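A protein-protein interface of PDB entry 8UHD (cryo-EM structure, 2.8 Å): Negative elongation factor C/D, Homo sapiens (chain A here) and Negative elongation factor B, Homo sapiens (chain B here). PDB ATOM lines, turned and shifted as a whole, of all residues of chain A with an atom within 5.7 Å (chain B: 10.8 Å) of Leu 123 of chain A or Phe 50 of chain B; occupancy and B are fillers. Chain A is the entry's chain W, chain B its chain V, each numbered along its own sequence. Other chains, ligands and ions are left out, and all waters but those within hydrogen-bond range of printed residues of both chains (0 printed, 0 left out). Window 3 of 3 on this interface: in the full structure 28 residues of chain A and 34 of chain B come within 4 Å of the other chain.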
ATOM      1  N   HIS A 118      15.827  33.778 -21.510  1.00  0.00           N
ATOM      2  CA  HIS A 118      17.134  34.327 -21.155  1.00  0.00           C
ATOM      3  C   HIS A 118      18.205  33.866 -22.136  1.00  0.00           C
ATOM      4  O   HIS A 118      18.986  34.680 -22.643  1.00  0.00           O
ATOM      5  CB  HIS A 118      17.515  33.924 -19.730  1.00  0.00           C
ATOM      6  CG  HIS A 118      16.609  34.476 -18.677  1.00  0.00           C
ATOM      7  ND1 HIS A 118      15.686  35.468 -18.929  1.00  0.00           N
ATOM      8  CD2 HIS A 118      16.499  34.187 -17.358  1.00  0.00           C
ATOM      9  CE1 HIS A 118      15.038  35.759 -17.814  1.00  0.00           C
ATOM     10  NE2 HIS A 118      15.517  34.999 -16.845  1.00  0.00           N
ATOM     11  N   LEU A 119      18.257  32.557 -22.408  1.00  0.00           N
ATOM     12  CA  LEU A 119      19.200  32.040 -23.400  1.00  0.00           C
ATOM     13  C   LEU A 119      18.948  32.673 -24.761  1.00  0.00           C
ATOM     14  O   LEU A 119      19.891  32.982 -25.500  1.00  0.00           O
ATOM     15  CB  LEU A 119      19.092  30.514 -23.481  1.00  0.00           C
ATOM     16  CG  LEU A 119      20.198  29.712 -24.195  1.00  0.00           C
ATOM     17  CD1 LEU A 119      20.159  28.258 -23.735  1.00  0.00           C
ATOM     18  CD2 LEU A 119      20.099  29.769 -25.726  1.00  0.00           C
ATOM     19  N   LYS A 120      17.677  32.904 -25.087  1.00  0.00           N
ATOM     20  CA  LYS A 120      17.315  33.524 -26.354  1.00  0.00           C
ATOM     21  C   LYS A 120      17.891  34.930 -26.465  1.00  0.00           C
ATOM     22  O   LYS A 120      18.519  35.279 -27.471  1.00  0.00           O
ATOM     23  CB  LYS A 120      15.792  33.556 -26.474  1.00  0.00           C
ATOM     24  CG  LYS A 120      15.297  33.640 -27.887  1.00  0.00           C
ATOM     25  CD  LYS A 120      13.779  33.487 -28.004  1.00  0.00           C
ATOM     26  CE  LYS A 120      13.291  32.080 -27.667  1.00  0.00           C
ATOM     27  NZ  LYS A 120      11.892  31.860 -28.121  1.00  0.00           N
ATOM     28  N   SER A 121      17.690  35.748 -25.431  1.00  0.00           N
ATOM     29  CA  SER A 121      18.202  37.114 -25.448  1.00  0.00           C
ATOM     30  C   SER A 121      19.725  37.132 -25.480  1.00  0.00           C
ATOM     31  O   SER A 121      20.330  37.931 -26.211  1.00  0.00           O
ATOM     32  CB  SER A 121      17.682  37.879 -24.231  1.00  0.00           C
ATOM     33  OG  SER A 121      17.882  37.140 -23.039  1.00  0.00           O
ATOM     34  N   LEU A 122      20.362  36.255 -24.696  1.00  0.00           N
ATOM     35  CA  LEU A 122      21.821  36.206 -24.674  1.00  0.00           C
ATOM     36  C   LEU A 122      22.379  35.830 -26.041  1.00  0.00           C
ATOM     37  O   LEU A 122      23.341  36.444 -26.513  1.00  0.00           O
ATOM     38  CB  LEU A 122      22.309  35.222 -23.607  1.00  0.00           C
ATOM     39  CG  LEU A 122      21.968  35.492 -22.128  1.00  0.00           C
ATOM     40  CD1 LEU A 122      22.035  34.193 -21.319  1.00  0.00           C
ATOM     41  CD2 LEU A 122      22.855  36.559 -21.481  1.00  0.00           C
ATOM     42  N   LEU A 123      21.775  34.839 -26.705  1.00  0.00           N
ATOM     43  CA  LEU A 123      22.234  34.465 -28.041  1.00  0.00           C
ATOM     44  C   LEU A 123      21.956  35.573 -29.049  1.00  0.00           C
ATOM     45  O   LEU A 123      22.746  35.780 -29.979  1.00  0.00           O
ATOM     46  CB  LEU A 123      21.570  33.162 -28.487  1.00  0.00           C
ATOM     47  CG  LEU A 123      22.157  32.498 -29.742  1.00  0.00           C
ATOM     48  CD1 LEU A 123      23.388  31.673 -29.396  1.00  0.00           C
ATOM     49  CD2 LEU A 123      21.116  31.644 -30.448  1.00  0.00           C
ATOM     50  N   ILE A 124      20.831  36.278 -28.897  1.00  0.00           N
ATOM     51  CA  ILE A 124      20.500  37.355 -29.826  1.00  0.00           C
ATOM     52  C   ILE A 124      21.546  38.461 -29.748  1.00  0.00           C
ATOM     53  O   ILE A 124      22.005  38.968 -30.778  1.00  0.00           O
ATOM     54  CB  ILE A 124      19.073  37.876 -29.548  1.00  0.00           C
ATOM     55  CG1 ILE A 124      18.047  36.876 -30.098  1.00  0.00           C
ATOM     56  CG2 ILE A 124      18.848  39.267 -30.175  1.00  0.00           C
ATOM     57  CD1 ILE A 124      16.637  37.023 -29.536  1.00  0.00           C
ATOM     58  N   LYS A 125      21.948  38.845 -28.533  1.00  0.00           N
ATOM     59  CA  LYS A 125      22.945  39.904 -28.398  1.00  0.00           C
ATOM     60  C   LYS A 125      24.381  39.413 -28.591  1.00  0.00           C
ATOM     61  O   LYS A 125      25.270  40.249 -28.789  1.00  0.00           O
ATOM     62  CB  LYS A 125      22.790  40.604 -27.040  1.00  0.00           C
ATOM     63  CG  LYS A 125      23.259  39.827 -25.823  1.00  0.00           C
ATOM     64  CD  LYS A 125      22.994  40.598 -24.542  1.00  0.00           C
ATOM     65  CE  LYS A 125      24.037  40.268 -23.491  1.00  0.00           C
ATOM     66  NZ  LYS A 125      24.160  38.803 -23.306  1.00  0.00           N
ATOM     67  N   HIS A 126      24.629  38.097 -28.542  1.00  0.00           N
ATOM     68  CA  HIS A 126      25.929  37.505 -28.860  1.00  0.00           C
ATOM     69  C   HIS A 126      25.942  36.837 -30.236  1.00  0.00           C
ATOM     70  O   HIS A 126      26.848  36.051 -30.534  1.00  0.00           O
ATOM     71  CB  HIS A 126      26.338  36.500 -27.774  1.00  0.00           C
ATOM     72  CG  HIS A 126      26.940  37.132 -26.558  1.00  0.00           C
ATOM     73  ND1 HIS A 126      26.389  38.228 -25.933  1.00  0.00           N
ATOM     74  CD2 HIS A 126      28.047  36.811 -25.846  1.00  0.00           C
ATOM     75  CE1 HIS A 126      27.133  38.562 -24.895  1.00  0.00           C
ATOM     76  NE2 HIS A 126      28.143  37.716 -24.817  1.00  0.00           N
ATOM     77  N   PHE A 127      24.974  37.150 -31.095  1.00  0.00           N
ATOM     78  CA  PHE A 127      24.889  36.475 -32.380  1.00  0.00           C
ATOM     79  C   PHE A 127      26.031  36.904 -33.295  1.00  0.00           C
ATOM     80  O   PHE A 127      26.534  38.028 -33.216  1.00  0.00           O
ATOM     81  CB  PHE A 127      23.545  36.766 -33.049  1.00  0.00           C
ATOM     82  CG  PHE A 127      23.226  35.846 -34.200  1.00  0.00           C
ATOM     83  CD1 PHE A 127      22.978  34.500 -33.983  1.00  0.00           C
ATOM     84  CD2 PHE A 127      23.177  36.330 -35.496  1.00  0.00           C
ATOM     85  CE1 PHE A 127      22.689  33.654 -35.036  1.00  0.00           C
ATOM     86  CE2 PHE A 127      22.886  35.488 -36.553  1.00  0.00           C
ATOM     87  CZ  PHE A 127      22.641  34.149 -36.323  1.00  0.00           C
ATOM     88  N   ASP A 128      26.440  35.977 -34.167  1.00  0.00           N
ATOM     89  CA  ASP A 128      27.514  36.213 -35.131  1.00  0.00           C
ATOM     90  C   ASP A 128      27.153  35.421 -36.392  1.00  0.00           C
ATOM     91  O   ASP A 128      27.326  34.192 -36.421  1.00  0.00           O
ATOM     92  CB  ASP A 128      28.870  35.780 -34.576  1.00  0.00           C
ATOM     93  CG  ASP A 128      30.047  36.402 -35.321  1.00  0.00           C
ATOM     94  OD1 ASP A 128      29.836  37.222 -36.240  1.00  0.00           O
ATOM     95  OD2 ASP A 128      31.199  36.065 -34.978  1.00  0.00           O
ATOM     96  N   TRP A 145      21.555  19.098 -33.530  1.00  0.00           N
ATOM     97  CA  TRP A 145      20.992  19.945 -32.483  1.00  0.00           C
ATOM     98  C   TRP A 145      19.995  20.946 -33.055  1.00  0.00           C
ATOM     99  O   TRP A 145      18.969  21.231 -32.427  1.00  0.00           O
ATOM    100  CB  TRP A 145      22.097  20.673 -31.706  1.00  0.00           C
ATOM    101  CG  TRP A 145      23.033  21.511 -32.534  1.00  0.00           C
ATOM    102  CD1 TRP A 145      24.251  21.137 -33.011  1.00  0.00           C
ATOM    103  CD2 TRP A 145      22.835  22.867 -32.963  1.00  0.00           C
ATOM    104  NE1 TRP A 145      24.823  22.165 -33.719  1.00  0.00           N
ATOM    105  CE2 TRP A 145      23.973  23.239 -33.706  1.00  0.00           C
ATOM    106  CE3 TRP A 145      21.806  23.799 -32.795  1.00  0.00           C
ATOM    107  CZ2 TRP A 145      24.109  24.502 -34.280  1.00  0.00           C
ATOM    108  CZ3 TRP A 145      21.938  25.046 -33.375  1.00  0.00           C
ATOM    109  CH2 TRP A 145      23.084  25.390 -34.101  1.00  0.00           C
ATOM    110  N   MET A 149      16.170  21.935 -32.076  1.00  0.00           N
ATOM    111  CA  MET A 149      15.658  23.287 -31.856  1.00  0.00           C
ATOM    112  C   MET A 149      14.426  23.555 -32.716  1.00  0.00           C
ATOM    113  O   MET A 149      13.491  24.235 -32.277  1.00  0.00           O
ATOM    114  CB  MET A 149      16.757  24.318 -32.134  1.00  0.00           C
ATOM    115  CG  MET A 149      18.071  24.162 -31.330  1.00  0.00           C
ATOM    116  SD  MET A 149      17.945  23.376 -29.703  1.00  0.00           S
ATOM    117  CE  MET A 149      19.550  22.589 -29.551  1.00  0.00           C
ATOM    118  N   TRP A 155      12.489  27.964 -29.998  1.00  0.00           N
ATOM    119  CA  TRP A 155      13.686  28.224 -30.788  1.00  0.00           C
ATOM    120  C   TRP A 155      13.339  28.522 -32.241  1.00  0.00           C
ATOM    121  O   TRP A 155      14.090  29.232 -32.919  1.00  0.00           O
ATOM    122  CB  TRP A 155      14.699  27.080 -30.724  1.00  0.00           C
ATOM    123  CG  TRP A 155      14.950  26.438 -29.377  1.00  0.00           C
ATOM    124  CD1 TRP A 155      14.084  25.703 -28.628  1.00  0.00           C
ATOM    125  CD2 TRP A 155      16.111  26.602 -28.579  1.00  0.00           C
ATOM    126  NE1 TRP A 155      14.660  25.339 -27.443  1.00  0.00           N
ATOM    127  CE2 TRP A 155      15.907  25.891 -27.380  1.00  0.00           C
ATOM    128  CE3 TRP A 155      17.316  27.273 -28.763  1.00  0.00           C
ATOM    129  CZ2 TRP A 155      16.869  25.824 -26.389  1.00  0.00           C
ATOM    130  CZ3 TRP A 155      18.262  27.197 -27.783  1.00  0.00           C
ATOM    131  CH2 TRP A 155      18.042  26.482 -26.611  1.00  0.00           C
ATOM    132  N   LEU A 158      12.891  32.074 -31.935  1.00  0.00           N
ATOM    133  CA  LEU A 158      14.222  32.674 -31.892  1.00  0.00           C
ATOM    134  C   LEU A 158      14.788  32.852 -33.292  1.00  0.00           C
ATOM    135  O   LEU A 158      15.298  33.922 -33.638  1.00  0.00           O
ATOM    136  CB  LEU A 158      15.164  31.808 -31.060  1.00  0.00           C
ATOM    137  CG  LEU A 158      16.683  32.053 -31.131  1.00  0.00           C
ATOM    138  CD1 LEU A 158      17.120  33.473 -30.753  1.00  0.00           C
ATOM    139  CD2 LEU A 158      17.359  31.048 -30.226  1.00  0.00           C
ATOM    140  N   LEU A 162      15.899  36.162 -35.343  1.00  0.00           N
ATOM    141  CA  LEU A 162      17.264  36.333 -35.830  1.00  0.00           C
ATOM    142  C   LEU A 162      17.280  36.658 -37.320  1.00  0.00           C
ATOM    143  O   LEU A 162      17.998  37.562 -37.761  1.00  0.00           O
ATOM    144  CB  LEU A 162      18.084  35.072 -35.548  1.00  0.00           C
ATOM    145  CG  LEU A 162      18.449  34.750 -34.095  1.00  0.00           C
ATOM    146  CD1 LEU A 162      19.068  33.363 -34.027  1.00  0.00           C
ATOM    147  CD2 LEU A 162      19.398  35.782 -33.501  1.00  0.00           C
ATOM    148  N   SER B  43      14.744  20.611 -21.465  1.00  0.00           N
ATOM    149  CA  SER B  43      15.086  21.524 -22.544  1.00  0.00           C
ATOM    150  C   SER B  43      16.579  21.858 -22.520  1.00  0.00           C
ATOM    151  O   SER B  43      17.247  21.946 -23.570  1.00  0.00           O
ATOM    152  CB  SER B  43      14.247  22.764 -22.402  1.00  0.00           C
ATOM    153  OG  SER B  43      14.721  23.505 -21.307  1.00  0.00           O
ATOM    154  N   LEU B  44      17.125  22.015 -21.319  1.00  0.00           N
ATOM    155  CA  LEU B  44      18.539  22.335 -21.199  1.00  0.00           C
ATOM    156  C   LEU B  44      19.389  21.177 -21.699  1.00  0.00           C
ATOM    157  O   LEU B  44      20.375  21.393 -22.390  1.00  0.00           O
ATOM    158  CB  LEU B  44      18.853  22.683 -19.756  1.00  0.00           C
ATOM    159  CG  LEU B  44      18.000  23.805 -19.139  1.00  0.00           C
ATOM    160  CD1 LEU B  44      18.381  23.965 -17.693  1.00  0.00           C
ATOM    161  CD2 LEU B  44      18.095  25.143 -19.877  1.00  0.00           C
ATOM    162  N   GLN B  45      18.995  19.929 -21.414  1.00  0.00           N
ATOM    163  CA  GLN B  45      19.809  18.799 -21.863  1.00  0.00           C
ATOM    164  C   GLN B  45      19.925  18.729 -23.380  1.00  0.00           C
ATOM    165  O   GLN B  45      20.905  18.170 -23.887  1.00  0.00           O
ATOM    166  CB  GLN B  45      19.248  17.467 -21.353  1.00  0.00           C
ATOM    167  CG  GLN B  45      18.930  17.412 -19.867  1.00  0.00           C
ATOM    168  CD  GLN B  45      19.924  18.170 -19.014  1.00  0.00           C
ATOM    169  OE1 GLN B  45      19.759  19.364 -18.776  1.00  0.00           O
ATOM    170  NE2 GLN B  45      20.958  17.482 -18.544  1.00  0.00           N
ATOM    171  N   SER B  46      18.964  19.290 -24.115  1.00  0.00           N
ATOM    172  CA  SER B  46      19.161  19.512 -25.539  1.00  0.00           C
ATOM    173  C   SER B  46      20.089  20.698 -25.795  1.00  0.00           C
ATOM    174  O   SER B  46      20.949  20.634 -26.683  1.00  0.00           O
ATOM    175  CB  SER B  46      17.819  19.751 -26.232  1.00  0.00           C
ATOM    176  OG  SER B  46      17.284  21.021 -25.901  1.00  0.00           O
ATOM    177  N   ALA B  47      19.937  21.785 -25.023  1.00  0.00           N
ATOM    178  CA  ALA B  47      20.564  23.059 -25.378  1.00  0.00           C
ATOM    179  C   ALA B  47      21.991  23.249 -24.864  1.00  0.00           C
ATOM    180  O   ALA B  47      22.707  24.099 -25.395  1.00  0.00           O
ATOM    181  CB  ALA B  47      19.718  24.219 -24.853  1.00  0.00           C
ATOM    182  N   LEU B  48      22.412  22.500 -23.847  1.00  0.00           N
ATOM    183  CA  LEU B  48      23.730  22.706 -23.240  1.00  0.00           C
ATOM    184  C   LEU B  48      24.884  22.465 -24.208  1.00  0.00           C
ATOM    185  O   LEU B  48      25.813  23.290 -24.230  1.00  0.00           O
ATOM    186  CB  LEU B  48      23.872  21.850 -21.970  1.00  0.00           C
ATOM    187  CG  LEU B  48      23.036  22.199 -20.725  1.00  0.00           C
ATOM    188  CD1 LEU B  48      23.262  21.166 -19.636  1.00  0.00           C
ATOM    189  CD2 LEU B  48      23.314  23.599 -20.190  1.00  0.00           C
ATOM    190  N   PRO B  49      24.919  21.387 -25.009  1.00  0.00           N
ATOM    191  CA  PRO B  49      25.984  21.314 -26.027  1.00  0.00           C
ATOM    192  C   PRO B  49      25.902  22.432 -27.051  1.00  0.00           C
ATOM    193  O   PRO B  49      26.934  22.997 -27.431  1.00  0.00           O
ATOM    194  CB  PRO B  49      25.774  19.934 -26.672  1.00  0.00           C
ATOM    195  CG  PRO B  49      24.884  19.189 -25.749  1.00  0.00           C
ATOM    196  CD  PRO B  49      24.029  20.216 -25.095  1.00  0.00           C
ATOM    197  N   PHE B  50      24.693  22.788 -27.494  1.00  0.00           N
ATOM    198  CA  PHE B  50      24.553  23.916 -28.410  1.00  0.00           C
ATOM    199  C   PHE B  50      24.967  25.219 -27.740  1.00  0.00           C
ATOM    200  O   PHE B  50      25.637  26.055 -28.359  1.00  0.00           O
ATOM    201  CB  PHE B  50      23.110  24.033 -28.904  1.00  0.00           C
ATOM    202  CG  PHE B  50      22.701  25.445 -29.228  1.00  0.00           C
ATOM    203  CD1 PHE B  50      23.118  26.035 -30.406  1.00  0.00           C
ATOM    204  CD2 PHE B  50      21.926  26.189 -28.350  1.00  0.00           C
ATOM    205  CE1 PHE B  50      22.756  27.329 -30.716  1.00  0.00           C
ATOM    206  CE2 PHE B  50      21.581  27.491 -28.649  1.00  0.00           C
ATOM    207  CZ  PHE B  50      21.992  28.059 -29.835  1.00  0.00           C
ATOM    208  N   LEU B  51      24.531  25.417 -26.491  1.00  0.00           N
ATOM    209  CA  LEU B  51      24.888  26.607 -25.726  1.00  0.00           C
ATOM    210  C   LEU B  51      26.394  26.743 -25.638  1.00  0.00           C
ATOM    211  O   LEU B  51      26.943  27.840 -25.795  1.00  0.00           O
ATOM    212  CB  LEU B  51      24.281  26.514 -24.319  1.00  0.00           C
ATOM    213  CG  LEU B  51      24.652  27.502 -23.196  1.00  0.00           C
ATOM    214  CD1 LEU B  51      23.967  28.845 -23.387  1.00  0.00           C
ATOM    215  CD2 LEU B  51      24.317  26.911 -21.830  1.00  0.00           C
ATOM    216  N   ASP B  52      27.072  25.627 -25.414  1.00  0.00           N
ATOM    217  CA  ASP B  52      28.502  25.607 -25.202  1.00  0.00           C
ATOM    218  C   ASP B  52      29.291  25.551 -26.511  1.00  0.00           C
ATOM    219  O   ASP B  52      30.516  25.711 -26.485  1.00  0.00           O
ATOM    220  CB  ASP B  52      28.832  24.391 -24.321  1.00  0.00           C
ATOM    221  CG  ASP B  52      30.117  24.542 -23.562  1.00  0.00           C
ATOM    222  OD1 ASP B  52      30.621  25.669 -23.511  1.00  0.00           O
ATOM    223  OD2 ASP B  52      30.619  23.539 -23.011  1.00  0.00           O
ATOM    224  N   LEU B  53      28.615  25.334 -27.647  1.00  0.00           N
ATOM    225  CA  LEU B  53      29.294  25.211 -28.935  1.00  0.00           C
ATOM    226  C   LEU B  53      30.027  26.487 -29.337  1.00  0.00           C
ATOM    227  O   LEU B  53      31.038  26.417 -30.046  1.00  0.00           O
ATOM    228  CB  LEU B  53      28.266  24.829 -30.006  1.00  0.00           C
ATOM    229  CG  LEU B  53      28.687  24.676 -31.473  1.00  0.00           C
ATOM    230  CD1 LEU B  53      29.595  23.472 -31.650  1.00  0.00           C
ATOM    231  CD2 LEU B  53      27.453  24.552 -32.357  1.00  0.00           C
ATOM    232  N   HIS B  54      29.549  27.653 -28.904  1.00  0.00           N
ATOM    233  CA  HIS B  54      30.102  28.927 -29.357  1.00  0.00           C
ATOM    234  C   HIS B  54      31.343  29.356 -28.585  1.00  0.00           C
ATOM    235  O   HIS B  54      31.739  30.523 -28.693  1.00  0.00           O
ATOM    236  CB  HIS B  54      29.056  30.041 -29.242  1.00  0.00           C
ATOM    237  CG  HIS B  54      27.713  29.679 -29.791  1.00  0.00           C
ATOM    238  ND1 HIS B  54      26.811  28.904 -29.094  1.00  0.00           N
ATOM    239  CD2 HIS B  54      27.111  29.995 -30.963  1.00  0.00           C
ATOM    240  CE1 HIS B  54      25.715  28.754 -29.815  1.00  0.00           C
ATOM    241  NE2 HIS B  54      25.871  29.406 -30.954  1.00  0.00           N
ATOM    242  N   GLY B  55      31.962  28.466 -27.811  1.00  0.00           N
ATOM    243  CA  GLY B  55      32.943  28.900 -26.840  1.00  0.00           C
ATOM    244  C   GLY B  55      32.353  29.597 -25.636  1.00  0.00           C
ATOM    245  O   GLY B  55      33.104  30.149 -24.826  1.00  0.00           O
ATOM    246  N   THR B  56      31.030  29.587 -25.491  1.00  0.00           N
ATOM    247  CA  THR B  56      30.377  30.260 -24.380  1.00  0.00           C
ATOM    248  C   THR B  56      30.567  29.420 -23.119  1.00  0.00           C
ATOM    249  O   THR B  56      30.143  28.260 -23.106  1.00  0.00           O
ATOM    250  CB  THR B  56      28.887  30.427 -24.670  1.00  0.00           C
ATOM    251  OG1 THR B  56      28.711  31.175 -25.880  1.00  0.00           O
ATOM    252  CG2 THR B  56      28.170  31.139 -23.523  1.00  0.00           C
ATOM    253  N   PRO B  57      31.174  29.940 -22.048  1.00  0.00           N
ATOM    254  CA  PRO B  57      31.302  29.109 -20.849  1.00  0.00           C
ATOM    255  C   PRO B  57      29.950  28.872 -20.206  1.00  0.00           C
ATOM    256  O   PRO B  57      29.053  29.717 -20.257  1.00  0.00           O
ATOM    257  CB  PRO B  57      32.216  29.921 -19.926  1.00  0.00           C
ATOM    258  CG  PRO B  57      32.320  31.275 -20.501  1.00  0.00           C
ATOM    259  CD  PRO B  57      31.527  31.344 -21.760  1.00  0.00           C
ATOM    260  N   ARG B  58      29.811  27.699 -19.589  1.00  0.00           N
ATOM    261  CA  ARG B  58      28.651  27.469 -18.741  1.00  0.00           C
ATOM    262  C   ARG B  58      28.694  28.317 -17.473  1.00  0.00           C
ATOM    263  O   ARG B  58      27.663  28.444 -16.809  1.00  0.00           O
ATOM    264  CB  ARG B  58      28.536  25.988 -18.370  1.00  0.00           C
ATOM    265  CG  ARG B  58      28.449  25.007 -19.550  1.00  0.00           C
ATOM    266  CD  ARG B  58      27.075  24.338 -19.644  1.00  0.00           C
ATOM    267  NE  ARG B  58      27.047  23.249 -20.619  1.00  0.00           N
ATOM    268  CZ  ARG B  58      27.440  21.999 -20.393  1.00  0.00           C
ATOM    269  NH1 ARG B  58      27.928  21.617 -19.220  1.00  0.00           N
ATOM    270  NH2 ARG B  58      27.341  21.103 -21.371  1.00  0.00           N
ATOM    271  N   GLU B  60      28.928  31.614 -17.212  1.00  0.00           N
ATOM    272  CA  GLU B  60      28.070  32.788 -17.359  1.00  0.00           C
ATOM    273  C   GLU B  60      26.606  32.404 -17.200  1.00  0.00           C
ATOM    274  O   GLU B  60      25.846  33.078 -16.491  1.00  0.00           O
ATOM    275  CB  GLU B  60      28.323  33.435 -18.723  1.00  0.00           C
ATOM    276  CG  GLU B  60      27.654  34.796 -18.946  1.00  0.00           C
ATOM    277  CD  GLU B  60      27.337  35.071 -20.409  1.00  0.00           C
ATOM    278  OE1 GLU B  60      27.937  34.425 -21.295  1.00  0.00           O
ATOM    279  OE2 GLU B  60      26.478  35.938 -20.672  1.00  0.00           O
ATOM    280  N   PHE B  61      26.203  31.306 -17.844  1.00  0.00           N
ATOM    281  CA  PHE B  61      24.832  30.819 -17.725  1.00  0.00           C
ATOM    282  C   PHE B  61      24.497  30.488 -16.276  1.00  0.00           C
ATOM    283  O   PHE B  61      23.482  30.958 -15.745  1.00  0.00           O
ATOM    284  CB  PHE B  61      24.644  29.600 -18.635  1.00  0.00           C
ATOM    285  CG  PHE B  61      23.526  28.682 -18.219  1.00  0.00           C
ATOM    286  CD1 PHE B  61      22.206  29.106 -18.239  1.00  0.00           C
ATOM    287  CD2 PHE B  61      23.798  27.380 -17.833  1.00  0.00           C
ATOM    288  CE1 PHE B  61      21.184  28.251 -17.861  1.00  0.00           C
ATOM    289  CE2 PHE B  61      22.782  26.524 -17.455  1.00  0.00           C
ATOM    290  CZ  PHE B  61      21.474  26.959 -17.471  1.00  0.00           C
ATOM    291  N   SER B  64      24.279  33.668 -14.075  1.00  0.00           N
ATOM    292  CA  SER B  64      23.121  34.508 -14.362  1.00  0.00           C
ATOM    293  C   SER B  64      21.843  33.893 -13.804  1.00  0.00           C
ATOM    294  O   SER B  64      21.066  34.568 -13.112  1.00  0.00           O
ATOM    295  CB  SER B  64      22.999  34.727 -15.870  1.00  0.00           C
ATOM    296  OG  SER B  64      22.783  33.502 -16.546  1.00  0.00           O
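Leu 123 of chain A touches just these residues of chain B: Phe 50 (3.7 Å) and His 54 (3.7 Å).
Of the printed residues of chain A, Phe 50 of chain B touches Leu 119 (3.99 Å), Leu 123 (3.7 Å), Trp 145 (3.3 Å), Met 149 (3.9 Å) and Trp 155 (3.4 Å).
No residue of chain B comes within 4 Å of Ser 121 of chain A.
Leu 122 of chain A touches just one residue of chain B: Glu 60.
Ile 124 of chain A touches none of the printed residues of chain B.
No residue of chain B comes within 4 Å of Phe 127 of chain A.
Of the printed residues of chain B, Leu 119 of chain A touches Phe 50 and Leu 51.
Of the printed residues of chain A, Glu 60 of chain B touches Leu 122.
Printed residues of chain B within 4 Å of Trp 155 of chain A: Ala 47 and Phe 50.
Gly 55 of chain B touches none of the printed residues of chain A.
Ser 64 of chain B touches none of the printed residues of chain A.
The nearest residue of chain B that does not touch Leu 123 of chain A is Leu 51 of chain B (6.3 Å).
The nearest printed residue of chain A that does not touch Leu 53 of chain B is Leu 123 of chain A (8.4 Å).
Leu 119 of chain A touches Phe 50 of chain B.
Leu 122 of chain A touches Glu 60 of chain B (CD2 to OE2, 3.8 Å).
CZ of Phe 50 of chain B touches CD2 of Leu 123 of chain A, at 3.7 Å.
Leu 123 of chain A touches His 54 of chain B (CD1 to NE2, 3.7 Å).
Trp 145 of chain A touches Phe 50 of chain B (CZ3 to CD1, 3.3 Å).
CD2 of Leu 53 of chain B touches NE1 of Trp 145 of chain A (3.8 Å).
Met 149 of chain A touches Ser 46 of chain B.
CE of Met 149 of chain A touches CB of Phe 50 of chain B (3.9 Å).
Ala 47 of chain B touches Trp 155 of chain A.
CZ3 of Trp 155 of chain A touches CE2 of Phe 50 of chain B, at 3.4 Å.
Of the 19 printed residues of chain B, 7 touch a printed residue of chain A.
Printed residues of chain B that touch a printed residue of chain A: Ser 46, Ala 47, Phe 50, Leu 51, Leu 53, His 54 and Glu 60.
Hydrophobic or aromatic side chains of chain A within 4 Å of the printed part of chain B: Leu 119, Leu 122, Leu 123, Trp 145, Met 149 and Trp 155.
Among the printed residues, 11 pairs touch across the chains.
O of Ser 43 of chain B lies within hydrogen-bond range of OG of Ser 46 of chain B, 2.5 Å away.
ND1 of His 54 of chain B sits close to O of Phe 50 of chain B.
A ring nitrogen (ND1) of His 54 of chain B sits at hydrogen-bond distance from the backbone carbonyl oxygen (O) of Leu 51 of chain B (3.5 Å).
O of Glu 60 of chain B lies within hydrogen-bond range of OG of Ser 64 of chain B (3.1 Å).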
